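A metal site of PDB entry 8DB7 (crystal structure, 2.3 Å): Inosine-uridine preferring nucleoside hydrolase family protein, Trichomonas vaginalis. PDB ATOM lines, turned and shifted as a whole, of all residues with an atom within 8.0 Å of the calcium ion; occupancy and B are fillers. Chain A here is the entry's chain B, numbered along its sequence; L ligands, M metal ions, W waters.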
ATOM      1  N   ASP A   6      16.559  -6.943  22.204  1.00  0.00           N
ATOM      2  CA  ASP A   6      16.852  -8.370  22.185  1.00  0.00           C
ATOM      3  C   ASP A   6      16.100  -9.022  21.029  1.00  0.00           C
ATOM      4  O   ASP A   6      14.872  -8.872  20.928  1.00  0.00           O
ATOM      5  CB  ASP A   6      16.468  -9.008  23.509  1.00  0.00           C
ATOM      6  CG  ASP A   6      16.950 -10.413  23.631  1.00  0.00           C
ATOM      7  OD1 ASP A   6      18.180 -10.611  23.748  1.00  0.00           O
ATOM      8  OD2 ASP A   6      16.103 -11.335  23.606  1.00  0.00           O
ATOM      9  N   THR A   7      16.813  -9.756  20.178  1.00  0.00           N
ATOM     10  CA  THR A   7      16.253 -10.178  18.903  1.00  0.00           C
ATOM     11  C   THR A   7      16.774 -11.551  18.490  1.00  0.00           C
ATOM     12  O   THR A   7      17.903 -11.937  18.805  1.00  0.00           O
ATOM     13  CB  THR A   7      16.586  -9.123  17.817  1.00  0.00           C
ATOM     14  OG1 THR A   7      16.137  -9.586  16.545  1.00  0.00           O
ATOM     15  CG2 THR A   7      18.066  -8.877  17.741  1.00  0.00           C
ATOM     16  N   ASP A   8      15.931 -12.305  17.773  1.00  0.00           N
ATOM     17  CA  ASP A   8      16.353 -13.491  17.025  1.00  0.00           C
ATOM     18  C   ASP A   8      16.324 -13.201  15.534  1.00  0.00           C
ATOM     19  O   ASP A   8      15.949 -14.042  14.728  1.00  0.00           O
ATOM     20  CB  ASP A   8      15.514 -14.732  17.362  1.00  0.00           C
ATOM     21  CG  ASP A   8      14.056 -14.590  16.977  1.00  0.00           C
ATOM     22  OD1 ASP A   8      13.605 -13.460  16.774  1.00  0.00           O
ATOM     23  OD2 ASP A   8      13.349 -15.622  16.878  1.00  0.00           O
ATOM     24  N   CYS A   9      16.762 -11.985  15.188  1.00  0.00           N
ATOM     25  CA  CYS A   9      16.674 -11.377  13.871  1.00  0.00           C
ATOM     26  C   CYS A   9      16.488 -12.391  12.756  1.00  0.00           C
ATOM     27  O   CYS A   9      17.457 -12.938  12.219  1.00  0.00           O
ATOM     28  CB  CYS A   9      17.878 -10.509  13.550  1.00  0.00           C
ATOM     29  SG  CYS A   9      17.592  -9.537  11.988  1.00  0.00           S
ATOM     30  N   GLY A  10      15.239 -12.686  12.488  1.00  0.00           N
ATOM     31  CA  GLY A  10      14.724 -13.033  11.219  1.00  0.00           C
ATOM     32  C   GLY A  10      14.100 -11.834  10.523  1.00  0.00           C
ATOM     33  O   GLY A  10      14.415 -10.660  10.803  1.00  0.00           O
ATOM     34  N   ILE A  11      13.166 -12.123   9.633  1.00  0.00           N
ATOM     35  CA  ILE A  11      12.728 -11.142   8.656  1.00  0.00           C
ATOM     36  C   ILE A  11      12.014  -9.976   9.344  1.00  0.00           C
ATOM     37  O   ILE A  11      12.330  -8.814   9.099  1.00  0.00           O
ATOM     38  CB  ILE A  11      11.840 -11.830   7.599  1.00  0.00           C
ATOM     39  CG1 ILE A  11      12.710 -12.818   6.805  1.00  0.00           C
ATOM     40  CG2 ILE A  11      11.217 -10.778   6.693  1.00  0.00           C
ATOM     41  CD1 ILE A  11      12.018 -14.073   6.392  1.00  0.00           C
ATOM     42  N   ASP A  12      11.040 -10.278  10.215  1.00  0.00           N
ATOM     43  CA  ASP A  12      10.244  -9.181  10.757  1.00  0.00           C
ATOM     44  C   ASP A  12      10.983  -8.441  11.865  1.00  0.00           C
ATOM     45  O   ASP A  12      10.754  -7.247  12.059  1.00  0.00           O
ATOM     46  CB  ASP A  12       8.869  -9.676  11.229  1.00  0.00           C
ATOM     47  CG  ASP A  12       8.924 -10.649  12.387  1.00  0.00           C
ATOM     48  OD1 ASP A  12       9.854 -11.497  12.448  1.00  0.00           O
ATOM     49  OD2 ASP A  12       8.038 -10.568  13.257  1.00  0.00           O
ATOM     50  N   ASP A  13      11.887  -9.136  12.562  1.00  0.00           N
ATOM     51  CA  ASP A  13      12.823  -8.452  13.466  1.00  0.00           C
ATOM     52  C   ASP A  13      13.591  -7.359  12.739  1.00  0.00           C
ATOM     53  O   ASP A  13      13.737  -6.238  13.238  1.00  0.00           O
ATOM     54  CB  ASP A  13      13.847  -9.438  14.056  1.00  0.00           C
ATOM     55  CG  ASP A  13      13.223 -10.567  14.881  1.00  0.00           C
ATOM     56  OD1 ASP A  13      12.722 -11.547  14.296  1.00  0.00           O
ATOM     57  OD2 ASP A  13      13.287 -10.508  16.123  1.00  0.00           O
ATOM     58  N   ALA A  14      14.155  -7.686  11.576  1.00  0.00           N
ATOM     59  CA  ALA A  14      14.994  -6.717  10.874  1.00  0.00           C
ATOM     60  C   ALA A  14      14.210  -5.432  10.603  1.00  0.00           C
ATOM     61  O   ALA A  14      14.715  -4.334  10.878  1.00  0.00           O
ATOM     62  CB  ALA A  14      15.536  -7.337   9.579  1.00  0.00           C
ATOM     63  N   ALA A  16      11.656  -4.399  12.355  1.00  0.00           N
ATOM     64  CA  ALA A  16      11.471  -3.780  13.661  1.00  0.00           C
ATOM     65  C   ALA A  16      12.613  -2.847  13.984  1.00  0.00           C
ATOM     66  O   ALA A  16      12.403  -1.738  14.493  1.00  0.00           O
ATOM     67  CB  ALA A  16      11.354  -4.850  14.754  1.00  0.00           C
ATOM     68  N   ILE A  34      19.915 -13.872  20.124  1.00  0.00           N
ATOM     69  CA  ILE A  34      19.533 -15.175  20.649  1.00  0.00           C
ATOM     70  C   ILE A  34      19.057 -16.040  19.498  1.00  0.00           C
ATOM     71  O   ILE A  34      18.411 -15.545  18.561  1.00  0.00           O
ATOM     72  CB  ILE A  34      18.459 -15.028  21.740  1.00  0.00           C
ATOM     73  CG1 ILE A  34      18.340 -16.313  22.550  1.00  0.00           C
ATOM     74  CG2 ILE A  34      17.131 -14.664  21.132  1.00  0.00           C
ATOM     75  CD1 ILE A  34      17.179 -16.274  23.404  1.00  0.00           C
ATOM     76  N   GLY A  36      16.591 -18.194  17.753  1.00  0.00           N
ATOM     77  CA  GLY A  36      15.179 -18.555  17.694  1.00  0.00           C
ATOM     78  C   GLY A  36      14.848 -18.987  16.272  1.00  0.00           C
ATOM     79  O   GLY A  36      14.928 -20.173  15.948  1.00  0.00           O
ATOM     80  N   ASN A  37      14.447 -18.018  15.452  1.00  0.00           N
ATOM     81  CA  ASN A  37      14.154 -18.249  14.041  1.00  0.00           C
ATOM     82  C   ASN A  37      15.284 -19.026  13.375  1.00  0.00           C
ATOM     83  O   ASN A  37      15.040 -19.866  12.495  1.00  0.00           O
ATOM     84  CB  ASN A  37      13.912 -16.901  13.339  1.00  0.00           C
ATOM     85  CG  ASN A  37      12.646 -16.201  13.828  1.00  0.00           C
ATOM     86  OD1 ASN A  37      11.635 -16.840  14.109  1.00  0.00           O
ATOM     87  ND2 ASN A  37      12.720 -14.873  13.940  1.00  0.00           N
ATOM     88  N   HIS A  80      11.764 -18.456   8.210  1.00  0.00           N
ATOM     89  CA  HIS A  80      12.516 -17.244   7.899  1.00  0.00           C
ATOM     90  C   HIS A  80      13.686 -17.528   6.971  1.00  0.00           C
ATOM     91  O   HIS A  80      14.592 -16.695   6.850  1.00  0.00           O
ATOM     92  CB  HIS A  80      13.008 -16.576   9.190  1.00  0.00           C
ATOM     93  CG  HIS A  80      11.911 -16.003  10.042  1.00  0.00           C
ATOM     94  ND1 HIS A  80      11.750 -14.639  10.235  1.00  0.00           N
ATOM     95  CD2 HIS A  80      10.955 -16.604  10.789  1.00  0.00           C
ATOM     96  CE1 HIS A  80      10.725 -14.438  11.043  1.00  0.00           C
ATOM     97  NE2 HIS A  80      10.223 -15.610  11.385  1.00  0.00           N
ATOM     98  N   CYS A 124      11.857  -6.520  23.341  1.00  0.00           N
ATOM     99  CA  CYS A 124      12.123  -7.953  23.198  1.00  0.00           C
ATOM    100  C   CYS A 124      11.384  -8.505  21.998  1.00  0.00           C
ATOM    101  O   CYS A 124      10.160  -8.378  21.922  1.00  0.00           O
ATOM    102  CB  CYS A 124      11.706  -8.723  24.452  1.00  0.00           C
ATOM    103  SG  CYS A 124      12.349  -8.076  25.971  1.00  0.00           S
ATOM    104  N   LEU A 125      12.104  -9.131  21.076  1.00  0.00           N
ATOM    105  CA  LEU A 125      11.502  -9.619  19.839  1.00  0.00           C
ATOM    106  C   LEU A 125      11.744 -11.103  19.650  1.00  0.00           C
ATOM    107  O   LEU A 125      11.737 -11.593  18.526  1.00  0.00           O
ATOM    108  CB  LEU A 125      12.056  -8.884  18.634  1.00  0.00           C
ATOM    109  CG  LEU A 125      12.100  -7.379  18.757  1.00  0.00           C
ATOM    110  CD1 LEU A 125      12.757  -6.892  17.479  1.00  0.00           C
ATOM    111  CD2 LEU A 125      10.665  -6.874  18.902  1.00  0.00           C
ATOM    112  N   ALA A 126      11.978 -11.834  20.727  1.00  0.00           N
ATOM    113  CA  ALA A 126      12.616 -13.137  20.596  1.00  0.00           C
ATOM    114  C   ALA A 126      12.180 -14.006  21.767  1.00  0.00           C
ATOM    115  O   ALA A 126      11.503 -13.516  22.684  1.00  0.00           O
ATOM    116  CB  ALA A 126      14.159 -13.003  20.554  1.00  0.00           C
ATOM    117  N   PRO A 127      12.506 -15.288  21.743  1.00  0.00           N
ATOM    118  CA  PRO A 127      12.349 -16.079  22.958  1.00  0.00           C
ATOM    119  C   PRO A 127      13.170 -15.445  24.074  1.00  0.00           C
ATOM    120  O   PRO A 127      14.242 -14.873  23.827  1.00  0.00           O
ATOM    121  CB  PRO A 127      12.862 -17.466  22.571  1.00  0.00           C
ATOM    122  CG  PRO A 127      12.726 -17.502  21.095  1.00  0.00           C
ATOM    123  CD  PRO A 127      13.018 -16.103  20.625  1.00  0.00           C
ATOM    124  N   MET A 151       7.206  -8.614  22.055  1.00  0.00           N
ATOM    125  CA  MET A 151       6.410  -9.359  21.086  1.00  0.00           C
ATOM    126  C   MET A 151       6.430 -10.816  21.523  1.00  0.00           C
ATOM    127  O   MET A 151       7.473 -11.458  21.524  1.00  0.00           O
ATOM    128  CB  MET A 151       6.951  -9.198  19.671  1.00  0.00           C
ATOM    129  CG  MET A 151       6.012  -9.760  18.603  1.00  0.00           C
ATOM    130  SD  MET A 151       5.935 -11.577  18.523  1.00  0.00           S
ATOM    131  CE  MET A 151       4.152 -11.876  18.553  1.00  0.00           C
ATOM    132  N   GLU A 166       2.369 -19.092  20.724  1.00  0.00           N
ATOM    133  CA  GLU A 166       3.120 -18.219  19.845  1.00  0.00           C
ATOM    134  C   GLU A 166       4.600 -18.605  19.887  1.00  0.00           C
ATOM    135  O   GLU A 166       5.108 -19.088  20.906  1.00  0.00           O
ATOM    136  CB  GLU A 166       2.905 -16.761  20.270  1.00  0.00           C
ATOM    137  CG  GLU A 166       3.696 -15.737  19.495  1.00  0.00           C
ATOM    138  CD  GLU A 166       5.076 -15.541  20.065  1.00  0.00           C
ATOM    139  OE1 GLU A 166       5.225 -15.669  21.310  1.00  0.00           O
ATOM    140  OE2 GLU A 166       6.024 -15.277  19.284  1.00  0.00           O
ATOM    141  N   PHE A 167       5.304 -18.362  18.774  1.00  0.00           N
ATOM    142  CA  PHE A 167       6.639 -18.934  18.608  1.00  0.00           C
ATOM    143  C   PHE A 167       7.608 -18.522  19.728  1.00  0.00           C
ATOM    144  O   PHE A 167       8.303 -19.366  20.294  1.00  0.00           O
ATOM    145  CB  PHE A 167       7.217 -18.569  17.242  1.00  0.00           C
ATOM    146  CG  PHE A 167       8.637 -18.995  17.082  1.00  0.00           C
ATOM    147  CD1 PHE A 167       8.936 -20.285  16.662  1.00  0.00           C
ATOM    148  CD2 PHE A 167       9.678 -18.127  17.385  1.00  0.00           C
ATOM    149  CE1 PHE A 167      10.251 -20.692  16.524  1.00  0.00           C
ATOM    150  CE2 PHE A 167      11.002 -18.519  17.244  1.00  0.00           C
ATOM    151  CZ  PHE A 167      11.297 -19.815  16.817  1.00  0.00           C
ATOM    152  N   ASN A 168       7.706 -17.216  20.034  1.00  0.00           N
ATOM    153  CA  ASN A 168       8.698 -16.775  21.019  1.00  0.00           C
ATOM    154  C   ASN A 168       8.476 -17.460  22.373  1.00  0.00           C
ATOM    155  O   ASN A 168       9.436 -17.872  23.045  1.00  0.00           O
ATOM    156  CB  ASN A 168       8.632 -15.265  21.212  1.00  0.00           C
ATOM    157  CG  ASN A 168       9.292 -14.505  20.089  1.00  0.00           C
ATOM    158  OD1 ASN A 168      10.160 -15.032  19.387  1.00  0.00           O
ATOM    159  ND2 ASN A 168       8.875 -13.243  19.902  1.00  0.00           N
ATOM    160  N   ALA A 238       4.466  -8.903  13.179  1.00  0.00           N
ATOM    161  CA  ALA A 238       4.518  -9.115  14.621  1.00  0.00           C
ATOM    162  C   ALA A 238       5.561  -8.216  15.281  1.00  0.00           C
ATOM    163  O   ALA A 238       5.221  -7.338  16.070  1.00  0.00           O
ATOM    164  CB  ALA A 238       4.801 -10.597  14.928  1.00  0.00           C
ATOM    165  N   ASP A 239       6.843  -8.414  14.939  1.00  0.00           N
ATOM    166  CA  ASP A 239       7.890  -7.605  15.574  1.00  0.00           C
ATOM    167  C   ASP A 239       7.782  -6.123  15.209  1.00  0.00           C
ATOM    168  O   ASP A 239       7.881  -5.285  16.118  1.00  0.00           O
ATOM    169  CB  ASP A 239       9.266  -8.173  15.227  1.00  0.00           C
ATOM    170  CG  ASP A 239       9.604  -9.424  16.024  1.00  0.00           C
ATOM    171  OD1 ASP A 239       8.905  -9.743  17.039  1.00  0.00           O
ATOM    172  OD2 ASP A 239      10.566 -10.089  15.616  1.00  0.00           O
ATOM    173  N   PRO A 240       7.585  -5.739  13.936  1.00  0.00           N
ATOM    174  CA  PRO A 240       7.415  -4.306  13.636  1.00  0.00           C
ATOM    175  C   PRO A 240       6.333  -3.647  14.466  1.00  0.00           C
ATOM    176  O   PRO A 240       6.524  -2.518  14.922  1.00  0.00           O
ATOM    177  CB  PRO A 240       7.066  -4.308  12.140  1.00  0.00           C
ATOM    178  CG  PRO A 240       7.749  -5.521  11.629  1.00  0.00           C
ATOM    179  CD  PRO A 240       7.610  -6.544  12.691  1.00  0.00           C
HETATM  180  C1  LIG L   1       8.028 -12.528  15.818  1.00  0.00           C
HETATM  181  O1  LIG L   1       8.817 -12.417  16.989  1.00  0.00           O
HETATM  182  C2  LIG L   1       7.599 -13.984  15.606  1.00  0.00           C
HETATM  183  O2  LIG L   1       8.477 -14.820  16.339  1.00  0.00           O
HETATM  184  C3  LIG L   1       6.143 -14.150  16.061  1.00  0.00           C
HETATM  185  O3  LIG L   1       5.863 -15.463  16.483  1.00  0.00           O
HETATM  186  C1  LG2 L   2       6.056 -12.676  10.903  1.00  0.00           C
HETATM  187  C2  LG2 L   2       5.905 -17.647  12.469  1.00  0.00           C
HETATM  188  C3  LG2 L   2       5.023 -19.838  12.832  1.00  0.00           C
HETATM  189  C4  LG2 L   2       4.131 -19.674  11.795  1.00  0.00           C
HETATM  190  C5  LG2 L   2       4.138 -18.492  11.098  1.00  0.00           C
HETATM  191  C6  LG2 L   2       5.018 -17.475  11.423  1.00  0.00           C
HETATM  192  C7  LG2 L   2       5.482 -14.983  11.025  1.00  0.00           C
HETATM  193  C8  LG2 L   2       6.574 -13.249  12.180  1.00  0.00           C
HETATM  194  C9  LG2 L   2       5.909 -18.829  13.186  1.00  0.00           C
HETATM  195  F1  LG2 L   2       5.002 -21.012  13.507  1.00  0.00           F
HETATM  196  N1  LG2 L   2       4.943 -16.258  10.632  1.00  0.00           N
HETATM  197  N2  LG2 L   2       6.227 -14.659  12.246  1.00  0.00           N
HETATM  198  N3  LG2 L   2       5.393 -13.758  10.211  1.00  0.00           N
HETATM  199 CA    CA M   1      11.470 -12.281  16.305  1.00  0.00          CA
HETATM  200  O   HOH W   1      10.469 -13.144  14.143  1.00  0.00           O
HETATM  201  O   HOH W   2      10.920 -14.673  17.000  1.00  0.00           O
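Residues that only touch the calcium ion: Asn 37.
Water W1 bridges the side-chain carboxylate of Asp 12 (2.4 Å) and the side-chain amide nitrogen of Asn 37 (2.8 Å).
Water W2 bridges the side-chain amide oxygen of Asn 168 and the side-chain carboxylate of Asp 8.
The calcium ion is bound by O of Leu 125 (2.3 Å), OD2 of Asp 239 (2.5 Å), OD1 of Asp 13 (2.5 Å), OD1 of Asp 8 (2.5 Å), water W1 (2.5 Å), OD2 of Asp 13 (2.5 Å), water W2 (2.6 Å) and O1 of LIG L1 (2.7 Å).
The calcium ion has eight donor atoms within binding distance.
The backbone NH (N) of Leu 125 lies within hydrogen-bond range of the backbone carbonyl oxygen (O) of Asp 6 (2.8 Å).
N of Asp 239 lies within hydrogen-bond range of OD2 of Asp 12 (3.0 Å).
ND2 of Asn 37 sits close to OD1 of Asp 13 (3.3 Å).
The backbone NH (N) of Gly 10 sits close to the side-chain carboxylate (OD1) of Asp 13, at 3.3 Å.
The side-chain carboxylate of Asp 13 lies close to the side-chain hydroxyl of Thr 7 (3.0 Å).
The backbone NH (N) of Asn 37 sits at hydrogen-bond distance from the side-chain carboxylate (OD2) of Asp 8 (3.0 Å).
A ring nitrogen (NE2) of His 80 lies within hydrogen-bond range of the side-chain amide oxygen (OD1) of Asn 37.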
